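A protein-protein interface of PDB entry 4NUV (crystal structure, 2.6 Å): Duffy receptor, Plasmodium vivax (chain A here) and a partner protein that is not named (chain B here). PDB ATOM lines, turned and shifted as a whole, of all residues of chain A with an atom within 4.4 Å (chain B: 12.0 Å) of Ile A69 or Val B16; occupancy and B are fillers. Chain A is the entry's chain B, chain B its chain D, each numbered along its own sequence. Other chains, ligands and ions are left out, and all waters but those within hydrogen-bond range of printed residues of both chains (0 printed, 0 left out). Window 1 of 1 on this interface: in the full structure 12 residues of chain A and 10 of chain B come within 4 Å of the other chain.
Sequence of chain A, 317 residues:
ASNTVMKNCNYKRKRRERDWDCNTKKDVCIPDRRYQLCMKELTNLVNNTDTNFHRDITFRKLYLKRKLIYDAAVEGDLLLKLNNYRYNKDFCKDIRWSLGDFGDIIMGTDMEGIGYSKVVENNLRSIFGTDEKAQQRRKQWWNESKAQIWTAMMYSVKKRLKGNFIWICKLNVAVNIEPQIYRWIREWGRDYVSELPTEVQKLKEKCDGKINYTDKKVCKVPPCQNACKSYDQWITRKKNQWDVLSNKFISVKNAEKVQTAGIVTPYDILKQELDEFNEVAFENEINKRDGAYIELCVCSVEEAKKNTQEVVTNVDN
OD1 of Asp B12 lies close to N of Glu B14 (3.4 Å). OD2 of Asp B12 sits close to N of Asp B15 (3.4 Å). The backbone carbonyl oxygen (O) of Glu B14 lies within hydrogen-bond range of the side-chain amide nitrogen (ND2) of Asn B18. The backbone carbonyl oxygen (O) of Val B16 sits at hydrogen-bond distance from the side-chain hydroxyl (OG) of Ser B20 (2.7 Å).
Of the 12 printed residues of chain A, 7 touch a printed residue of chain B. Printed residues of chain B that touch a printed residue of chain A: Leu B11, Phe B13, Glu B14, Asp B15, Val B16, Trp B17, Ser B20 and Tyr B21. Hydrophobic or aromatic side chains of chain B within 4 Å of the printed part of chain A: Leu B11, Phe B13, Val B16, Trp B17 and Tyr B21. Among the printed residues, Asp or Glu carboxylates within 4 Å of a Lys or Arg side-chain nitrogen of the other chain: Arg A66 with Glu B14 (3.6 Å).
Ile A69 touches just these residues of chain B: Val B16 (3.9 Å), Trp B17 (3.7 Å) and Ser B20 (3.2 Å). Val B16 touches just these residues of chain A: Ile A69 (3.9 Å), Ala A73 (3.5 Å) and Tyr A155 (3.6 Å). Lys A65 touches one residue of chain B. No residue of chain B comes within 4 Å of Leu A68. No residue of chain B comes within 4 Å of Ala A72. Ala A73 touches one residue of chain B. No residue of chain B comes within 4 Å of Ile A149. Ala A152 touches just one residue of chain B: Ser B20. Printed residues of chain B within 4 Å of Tyr A155: Asp B15 (2.7 Å) and Val B16 (3.6 Å). Of the printed residues of chain A, Asp B15 touches Tyr A155. Of the printed residues of chain A, Ser B20 touches Ile A69 (3.2 Å) and Ala A152 (3.9 Å). Of the printed residues of chain B, Arg A66 touches Phe B13 (3.4 Å), Glu B14 (3.6 Å) and Trp B17 (3.5 Å). Asp B12 touches none of the printed residues of chain A.
Phe B13 touches Arg A66 (CZ to CG, 3.4 Å). Arg A66 touches Trp B17 (CA to CZ3, 3.5 Å). CG1 of Val B16 touches CG2 of Ile A69, at 3.9 Å. CD1 of Ile A69 touches CZ3 of Trp B17 (3.7 Å). Ile A69 touches Ser B20 (CG2 to OG, 3.2 Å). Tyr A70 touches Phe B13 (CD1 to CD2, 3.1 Å). Val B16 touches Ala A73. Ala A152 touches Ser B20. Val B16 touches Tyr A155.
OH of Tyr B21 lies within hydrogen-bond range of NZ of Lys A65 (3.3 Å). NH2 of Arg A66 lies within salt-bridge range of OE1 of Glu B14. O of Leu B11 is in hydrogen-bond range of OH of Tyr A70, 3.4 Å away. OH of Tyr A155 lies within hydrogen-bond range of OD2 of Asp B15, 2.7 Å away.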
ATOM      1  N   LYS A  65      23.855  15.980  32.228  1.00  0.00           N
ATOM      2  CA  LYS A  65      22.407  15.889  32.089  1.00  0.00           C
ATOM      3  C   LYS A  65      21.868  17.057  31.273  1.00  0.00           C
ATOM      4  O   LYS A  65      20.912  16.906  30.515  1.00  0.00           O
ATOM      5  CB  LYS A  65      21.728  15.864  33.460  1.00  0.00           C
ATOM      6  CG  LYS A  65      20.224  15.669  33.386  1.00  0.00           C
ATOM      7  CD  LYS A  65      19.617  15.431  34.757  1.00  0.00           C
ATOM      8  CE  LYS A  65      19.748  16.654  35.645  1.00  0.00           C
ATOM      9  NZ  LYS A  65      19.042  16.474  36.943  1.00  0.00           N
ATOM     10  N   ARG A  66      22.488  18.221  31.435  1.00  0.00           N
ATOM     11  CA  ARG A  66      22.072  19.417  30.710  1.00  0.00           C
ATOM     12  C   ARG A  66      22.194  19.221  29.203  1.00  0.00           C
ATOM     13  O   ARG A  66      21.278  19.551  28.453  1.00  0.00           O
ATOM     14  CB  ARG A  66      22.906  20.622  31.148  1.00  0.00           C
ATOM     15  CG  ARG A  66      22.572  21.898  30.398  1.00  0.00           C
ATOM     16  CD  ARG A  66      23.293  23.102  30.978  1.00  0.00           C
ATOM     17  NE  ARG A  66      22.785  24.358  30.430  1.00  0.00           N
ATOM     18  CZ  ARG A  66      23.271  25.561  30.721  1.00  0.00           C
ATOM     19  NH1 ARG A  66      24.294  25.691  31.556  1.00  0.00           N
ATOM     20  NH2 ARG A  66      22.733  26.640  30.169  1.00  0.00           N
ATOM     21  N   LYS A  67      23.325  18.683  28.764  1.00  0.00           N
ATOM     22  CA  LYS A  67      23.561  18.478  27.341  1.00  0.00           C
ATOM     23  C   LYS A  67      22.748  17.302  26.804  1.00  0.00           C
ATOM     24  O   LYS A  67      22.341  17.301  25.644  1.00  0.00           O
ATOM     25  CB  LYS A  67      25.050  18.256  27.074  1.00  0.00           C
ATOM     26  CG  LYS A  67      25.926  19.455  27.403  1.00  0.00           C
ATOM     27  CD  LYS A  67      25.375  20.734  26.787  1.00  0.00           C
ATOM     28  CE  LYS A  67      26.336  21.900  26.960  1.00  0.00           C
ATOM     29  NZ  LYS A  67      25.742  23.186  26.496  1.00  0.00           N
ATOM     30  N   LEU A  68      22.511  16.305  27.649  1.00  0.00           N
ATOM     31  CA  LEU A  68      21.753  15.131  27.237  1.00  0.00           C
ATOM     32  C   LEU A  68      20.284  15.494  27.055  1.00  0.00           C
ATOM     33  O   LEU A  68      19.635  15.052  26.108  1.00  0.00           O
ATOM     34  CB  LEU A  68      21.887  14.011  28.270  1.00  0.00           C
ATOM     35  CG  LEU A  68      21.196  12.695  27.904  1.00  0.00           C
ATOM     36  CD1 LEU A  68      21.784  12.120  26.626  1.00  0.00           C
ATOM     37  CD2 LEU A  68      21.302  11.688  29.041  1.00  0.00           C
ATOM     38  N   ILE A  69      19.769  16.306  27.971  1.00  0.00           N
ATOM     39  CA  ILE A  69      18.379  16.738  27.915  1.00  0.00           C
ATOM     40  C   ILE A  69      18.092  17.503  26.629  1.00  0.00           C
ATOM     41  O   ILE A  69      17.027  17.347  26.031  1.00  0.00           O
ATOM     42  CB  ILE A  69      18.020  17.619  29.124  1.00  0.00           C
ATOM     43  CG1 ILE A  69      17.729  16.740  30.342  1.00  0.00           C
ATOM     44  CG2 ILE A  69      16.808  18.493  28.813  1.00  0.00           C
ATOM     45  CD1 ILE A  69      17.530  17.515  31.628  1.00  0.00           C
ATOM     46  N   TYR A  70      19.041  18.331  26.205  1.00  0.00           N
ATOM     47  CA  TYR A  70      18.855  19.112  24.989  1.00  0.00           C
ATOM     48  C   TYR A  70      18.917  18.225  23.750  1.00  0.00           C
ATOM     49  O   TYR A  70      18.112  18.379  22.835  1.00  0.00           O
ATOM     50  CB  TYR A  70      19.888  20.234  24.891  1.00  0.00           C
ATOM     51  CG  TYR A  70      19.607  21.192  23.755  1.00  0.00           C
ATOM     52  CD1 TYR A  70      18.505  22.040  23.793  1.00  0.00           C
ATOM     53  CD2 TYR A  70      20.437  21.246  22.642  1.00  0.00           C
ATOM     54  CE1 TYR A  70      18.239  22.916  22.756  1.00  0.00           C
ATOM     55  CE2 TYR A  70      20.179  22.120  21.601  1.00  0.00           C
ATOM     56  CZ  TYR A  70      19.078  22.951  21.663  1.00  0.00           C
ATOM     57  OH  TYR A  70      18.818  23.821  20.631  1.00  0.00           O
ATOM     58  N   ASP A  71      19.871  17.299  23.724  1.00  0.00           N
ATOM     59  CA  ASP A  71      19.983  16.359  22.614  1.00  0.00           C
ATOM     60  C   ASP A  71      18.743  15.476  22.524  1.00  0.00           C
ATOM     61  O   ASP A  71      18.342  15.059  21.438  1.00  0.00           O
ATOM     62  CB  ASP A  71      21.229  15.483  22.767  1.00  0.00           C
ATOM     63  CG  ASP A  71      22.467  16.111  22.155  1.00  0.00           C
ATOM     64  OD1 ASP A  71      22.327  17.042  21.333  1.00  0.00           O
ATOM     65  OD2 ASP A  71      23.584  15.663  22.487  1.00  0.00           O
ATOM     66  N   ALA A  72      18.143  15.190  23.674  1.00  0.00           N
ATOM     67  CA  ALA A  72      16.948  14.362  23.727  1.00  0.00           C
ATOM     68  C   ALA A  72      15.761  15.096  23.108  1.00  0.00           C
ATOM     69  O   ALA A  72      14.964  14.504  22.382  1.00  0.00           O
ATOM     70  CB  ALA A  72      16.644  13.977  25.164  1.00  0.00           C
ATOM     71  N   ALA A  73      15.649  16.387  23.398  1.00  0.00           N
ATOM     72  CA  ALA A  73      14.550  17.192  22.880  1.00  0.00           C
ATOM     73  C   ALA A  73      14.652  17.355  21.368  1.00  0.00           C
ATOM     74  O   ALA A  73      13.638  17.394  20.670  1.00  0.00           O
ATOM     75  CB  ALA A  73      14.531  18.552  23.556  1.00  0.00           C
ATOM     76  N   ILE A 149      14.888  12.456  30.895  1.00  0.00           N
ATOM     77  CA  ILE A 149      15.364  12.398  29.519  1.00  0.00           C
ATOM     78  C   ILE A 149      14.187  12.101  28.591  1.00  0.00           C
ATOM     79  O   ILE A 149      14.011  12.754  27.560  1.00  0.00           O
ATOM     80  CB  ILE A 149      16.449  11.315  29.339  1.00  0.00           C
ATOM     81  CG1 ILE A 149      17.615  11.549  30.308  1.00  0.00           C
ATOM     82  CG2 ILE A 149      16.955  11.297  27.906  1.00  0.00           C
ATOM     83  CD1 ILE A 149      18.246  12.923  30.206  1.00  0.00           C
ATOM     84  N   ALA A 152      12.130  15.016  28.239  1.00  0.00           N
ATOM     85  CA  ALA A 152      12.800  15.971  27.369  1.00  0.00           C
ATOM     86  C   ALA A 152      12.546  15.631  25.901  1.00  0.00           C
ATOM     87  O   ALA A 152      12.394  16.524  25.072  1.00  0.00           O
ATOM     88  CB  ALA A 152      14.295  15.996  27.664  1.00  0.00           C
ATOM     89  N   TYR A 155       9.269  16.882  24.486  1.00  0.00           N
ATOM     90  CA  TYR A 155       9.140  18.332  24.581  1.00  0.00           C
ATOM     91  C   TYR A 155       8.166  18.900  23.548  1.00  0.00           C
ATOM     92  O   TYR A 155       7.230  19.615  23.899  1.00  0.00           O
ATOM     93  CB  TYR A 155      10.509  18.997  24.430  1.00  0.00           C
ATOM     94  CG  TYR A 155      10.439  20.501  24.326  1.00  0.00           C
ATOM     95  CD1 TYR A 155      10.289  21.290  25.458  1.00  0.00           C
ATOM     96  CD2 TYR A 155      10.519  21.133  23.094  1.00  0.00           C
ATOM     97  CE1 TYR A 155      10.222  22.666  25.365  1.00  0.00           C
ATOM     98  CE2 TYR A 155      10.455  22.508  22.990  1.00  0.00           C
ATOM     99  CZ  TYR A 155      10.305  23.270  24.129  1.00  0.00           C
ATOM    100  OH  TYR A 155      10.240  24.640  24.028  1.00  0.00           O
ATOM    101  N   GLN B  10      16.472  26.273  16.329  1.00  0.00           N
ATOM    102  CA  GLN B  10      15.085  26.717  16.365  1.00  0.00           C
ATOM    103  C   GLN B  10      14.369  26.156  17.589  1.00  0.00           C
ATOM    104  O   GLN B  10      13.143  26.030  17.602  1.00  0.00           O
ATOM    105  CB  GLN B  10      14.360  26.285  15.090  1.00  0.00           C
ATOM    106  CG  GLN B  10      14.344  24.780  14.871  1.00  0.00           C
ATOM    107  CD  GLN B  10      13.571  24.367  13.631  1.00  0.00           C
ATOM    108  OE1 GLN B  10      12.843  23.375  13.646  1.00  0.00           O
ATOM    109  NE2 GLN B  10      13.733  25.120  12.546  1.00  0.00           N
ATOM    110  N   LEU B  11      15.143  25.821  18.617  1.00  0.00           N
ATOM    111  CA  LEU B  11      14.592  25.286  19.857  1.00  0.00           C
ATOM    112  C   LEU B  11      15.160  26.021  21.065  1.00  0.00           C
ATOM    113  O   LEU B  11      16.367  26.004  21.302  1.00  0.00           O
ATOM    114  CB  LEU B  11      14.895  23.792  19.971  1.00  0.00           C
ATOM    115  CG  LEU B  11      14.128  22.877  19.014  1.00  0.00           C
ATOM    116  CD1 LEU B  11      14.678  21.462  19.079  1.00  0.00           C
ATOM    117  CD2 LEU B  11      12.643  22.887  19.337  1.00  0.00           C
ATOM    118  N   ASP B  12      14.279  26.661  21.827  1.00  0.00           N
ATOM    119  CA  ASP B  12      14.686  27.405  23.014  1.00  0.00           C
ATOM    120  C   ASP B  12      15.217  26.459  24.084  1.00  0.00           C
ATOM    121  O   ASP B  12      14.448  25.775  24.757  1.00  0.00           O
ATOM    122  CB  ASP B  12      13.511  28.209  23.569  1.00  0.00           C
ATOM    123  CG  ASP B  12      13.855  28.934  24.854  1.00  0.00           C
ATOM    124  OD1 ASP B  12      15.050  29.229  25.070  1.00  0.00           O
ATOM    125  OD2 ASP B  12      12.931  29.213  25.646  1.00  0.00           O
ATOM    126  N   PHE B  13      16.537  26.435  24.239  1.00  0.00           N
ATOM    127  CA  PHE B  13      17.189  25.527  25.173  1.00  0.00           C
ATOM    128  C   PHE B  13      16.611  25.634  26.581  1.00  0.00           C
ATOM    129  O   PHE B  13      16.279  24.625  27.202  1.00  0.00           O
ATOM    130  CB  PHE B  13      18.691  25.812  25.223  1.00  0.00           C
ATOM    131  CG  PHE B  13      19.462  24.838  26.065  1.00  0.00           C
ATOM    132  CD1 PHE B  13      19.358  24.860  27.446  1.00  0.00           C
ATOM    133  CD2 PHE B  13      20.291  23.900  25.475  1.00  0.00           C
ATOM    134  CE1 PHE B  13      20.062  23.964  28.218  1.00  0.00           C
ATOM    135  CE2 PHE B  13      20.999  23.002  26.244  1.00  0.00           C
ATOM    136  CZ  PHE B  13      20.885  23.034  27.617  1.00  0.00           C
ATOM    137  N   GLU B  14      16.499  26.858  27.083  1.00  0.00           N
ATOM    138  CA  GLU B  14      16.077  27.085  28.463  1.00  0.00           C
ATOM    139  C   GLU B  14      14.690  26.522  28.759  1.00  0.00           C
ATOM    140  O   GLU B  14      14.483  25.893  29.796  1.00  0.00           O
ATOM    141  CB  GLU B  14      16.119  28.578  28.791  1.00  0.00           C
ATOM    142  CG  GLU B  14      17.526  29.150  28.843  1.00  0.00           C
ATOM    143  CD  GLU B  14      18.380  28.499  29.917  1.00  0.00           C
ATOM    144  OE1 GLU B  14      19.616  28.445  29.746  1.00  0.00           O
ATOM    145  OE2 GLU B  14      17.815  28.044  30.934  1.00  0.00           O
ATOM    146  N   ASP B  15      13.740  26.747  27.858  1.00  0.00           N
ATOM    147  CA  ASP B  15      12.384  26.248  28.054  1.00  0.00           C
ATOM    148  C   ASP B  15      12.361  24.722  28.080  1.00  0.00           C
ATOM    149  O   ASP B  15      11.599  24.116  28.834  1.00  0.00           O
ATOM    150  CB  ASP B  15      11.453  26.769  26.960  1.00  0.00           C
ATOM    151  CG  ASP B  15      10.014  26.349  27.175  1.00  0.00           C
ATOM    152  OD1 ASP B  15       9.579  26.293  28.345  1.00  0.00           O
ATOM    153  OD2 ASP B  15       9.316  26.073  26.177  1.00  0.00           O
ATOM    154  N   VAL B  16      13.197  24.107  27.248  1.00  0.00           N
ATOM    155  CA  VAL B  16      13.345  22.655  27.242  1.00  0.00           C
ATOM    156  C   VAL B  16      13.846  22.176  28.595  1.00  0.00           C
ATOM    157  O   VAL B  16      13.331  21.211  29.160  1.00  0.00           O
ATOM    158  CB  VAL B  16      14.343  22.198  26.159  1.00  0.00           C
ATOM    159  CG1 VAL B  16      14.698  20.728  26.341  1.00  0.00           C
ATOM    160  CG2 VAL B  16      13.775  22.449  24.769  1.00  0.00           C
ATOM    161  N   TRP B  17      14.864  22.859  29.106  1.00  0.00           N
ATOM    162  CA  TRP B  17      15.445  22.525  30.397  1.00  0.00           C
ATOM    163  C   TRP B  17      14.418  22.692  31.515  1.00  0.00           C
ATOM    164  O   TRP B  17      14.253  21.807  32.353  1.00  0.00           O
ATOM    165  CB  TRP B  17      16.672  23.404  30.651  1.00  0.00           C
ATOM    166  CG  TRP B  17      17.196  23.330  32.045  1.00  0.00           C
ATOM    167  CD1 TRP B  17      16.949  24.208  33.057  1.00  0.00           C
ATOM    168  CD2 TRP B  17      18.061  22.326  32.585  1.00  0.00           C
ATOM    169  NE1 TRP B  17      17.606  23.814  34.194  1.00  0.00           N
ATOM    170  CE2 TRP B  17      18.297  22.660  33.932  1.00  0.00           C
ATOM    171  CE3 TRP B  17      18.659  21.175  32.062  1.00  0.00           C
ATOM    172  CZ2 TRP B  17      19.102  21.888  34.763  1.00  0.00           C
ATOM    173  CZ3 TRP B  17      19.460  20.409  32.889  1.00  0.00           C
ATOM    174  CH2 TRP B  17      19.675  20.769  34.225  1.00  0.00           C
ATOM    175  N   ASN B  18      13.722  23.824  31.515  1.00  0.00           N
ATOM    176  CA  ASN B  18      12.721  24.110  32.538  1.00  0.00           C
ATOM    177  C   ASN B  18      11.553  23.128  32.489  1.00  0.00           C
ATOM    178  O   ASN B  18      11.018  22.734  33.524  1.00  0.00           O
ATOM    179  CB  ASN B  18      12.199  25.540  32.381  1.00  0.00           C
ATOM    180  CG  ASN B  18      13.276  26.583  32.609  1.00  0.00           C
ATOM    181  OD1 ASN B  18      14.155  26.412  33.456  1.00  0.00           O
ATOM    182  ND2 ASN B  18      13.216  27.669  31.848  1.00  0.00           N
ATOM    183  N   SER B  19      11.163  22.738  31.280  1.00  0.00           N
ATOM    184  CA  SER B  19      10.055  21.810  31.093  1.00  0.00           C
ATOM    185  C   SER B  19      10.411  20.403  31.568  1.00  0.00           C
ATOM    186  O   SER B  19       9.539  19.643  31.988  1.00  0.00           O
ATOM    187  CB  SER B  19       9.653  21.765  29.620  1.00  0.00           C
ATOM    188  OG  SER B  19       8.576  20.868  29.418  1.00  0.00           O
ATOM    189  N   SER B  20      11.694  20.063  31.502  1.00  0.00           N
ATOM    190  CA  SER B  20      12.161  18.736  31.891  1.00  0.00           C
ATOM    191  C   SER B  20      11.856  18.425  33.356  1.00  0.00           C
ATOM    192  O   SER B  20      11.906  17.268  33.775  1.00  0.00           O
ATOM    193  CB  SER B  20      13.664  18.612  31.641  1.00  0.00           C
ATOM    194  OG  SER B  20      13.981  18.892  30.288  1.00  0.00           O
ATOM    195  N   TYR B  21      11.545  19.460  34.132  1.00  0.00           N
ATOM    196  CA  TYR B  21      11.184  19.284  35.534  1.00  0.00           C
ATOM    197  C   TYR B  21       9.711  19.610  35.755  1.00  0.00           C
ATOM    198  O   TYR B  21       8.837  18.791  35.479  1.00  0.00           O
ATOM    199  CB  TYR B  21      12.049  20.177  36.421  1.00  0.00           C
ATOM    200  CG  TYR B  21      13.529  19.934  36.266  1.00  0.00           C
ATOM    201  CD1 TYR B  21      14.176  18.966  37.021  1.00  0.00           C
ATOM    202  CD2 TYR B  21      14.282  20.672  35.363  1.00  0.00           C
ATOM    203  CE1 TYR B  21      15.529  18.741  36.883  1.00  0.00           C
ATOM    204  CE2 TYR B  21      15.636  20.454  35.218  1.00  0.00           C
ATOM    205  CZ  TYR B  21      16.255  19.487  35.980  1.00  0.00           C
ATOM    206  OH  TYR B  21      17.605  19.267  35.839  1.00  0.00           O
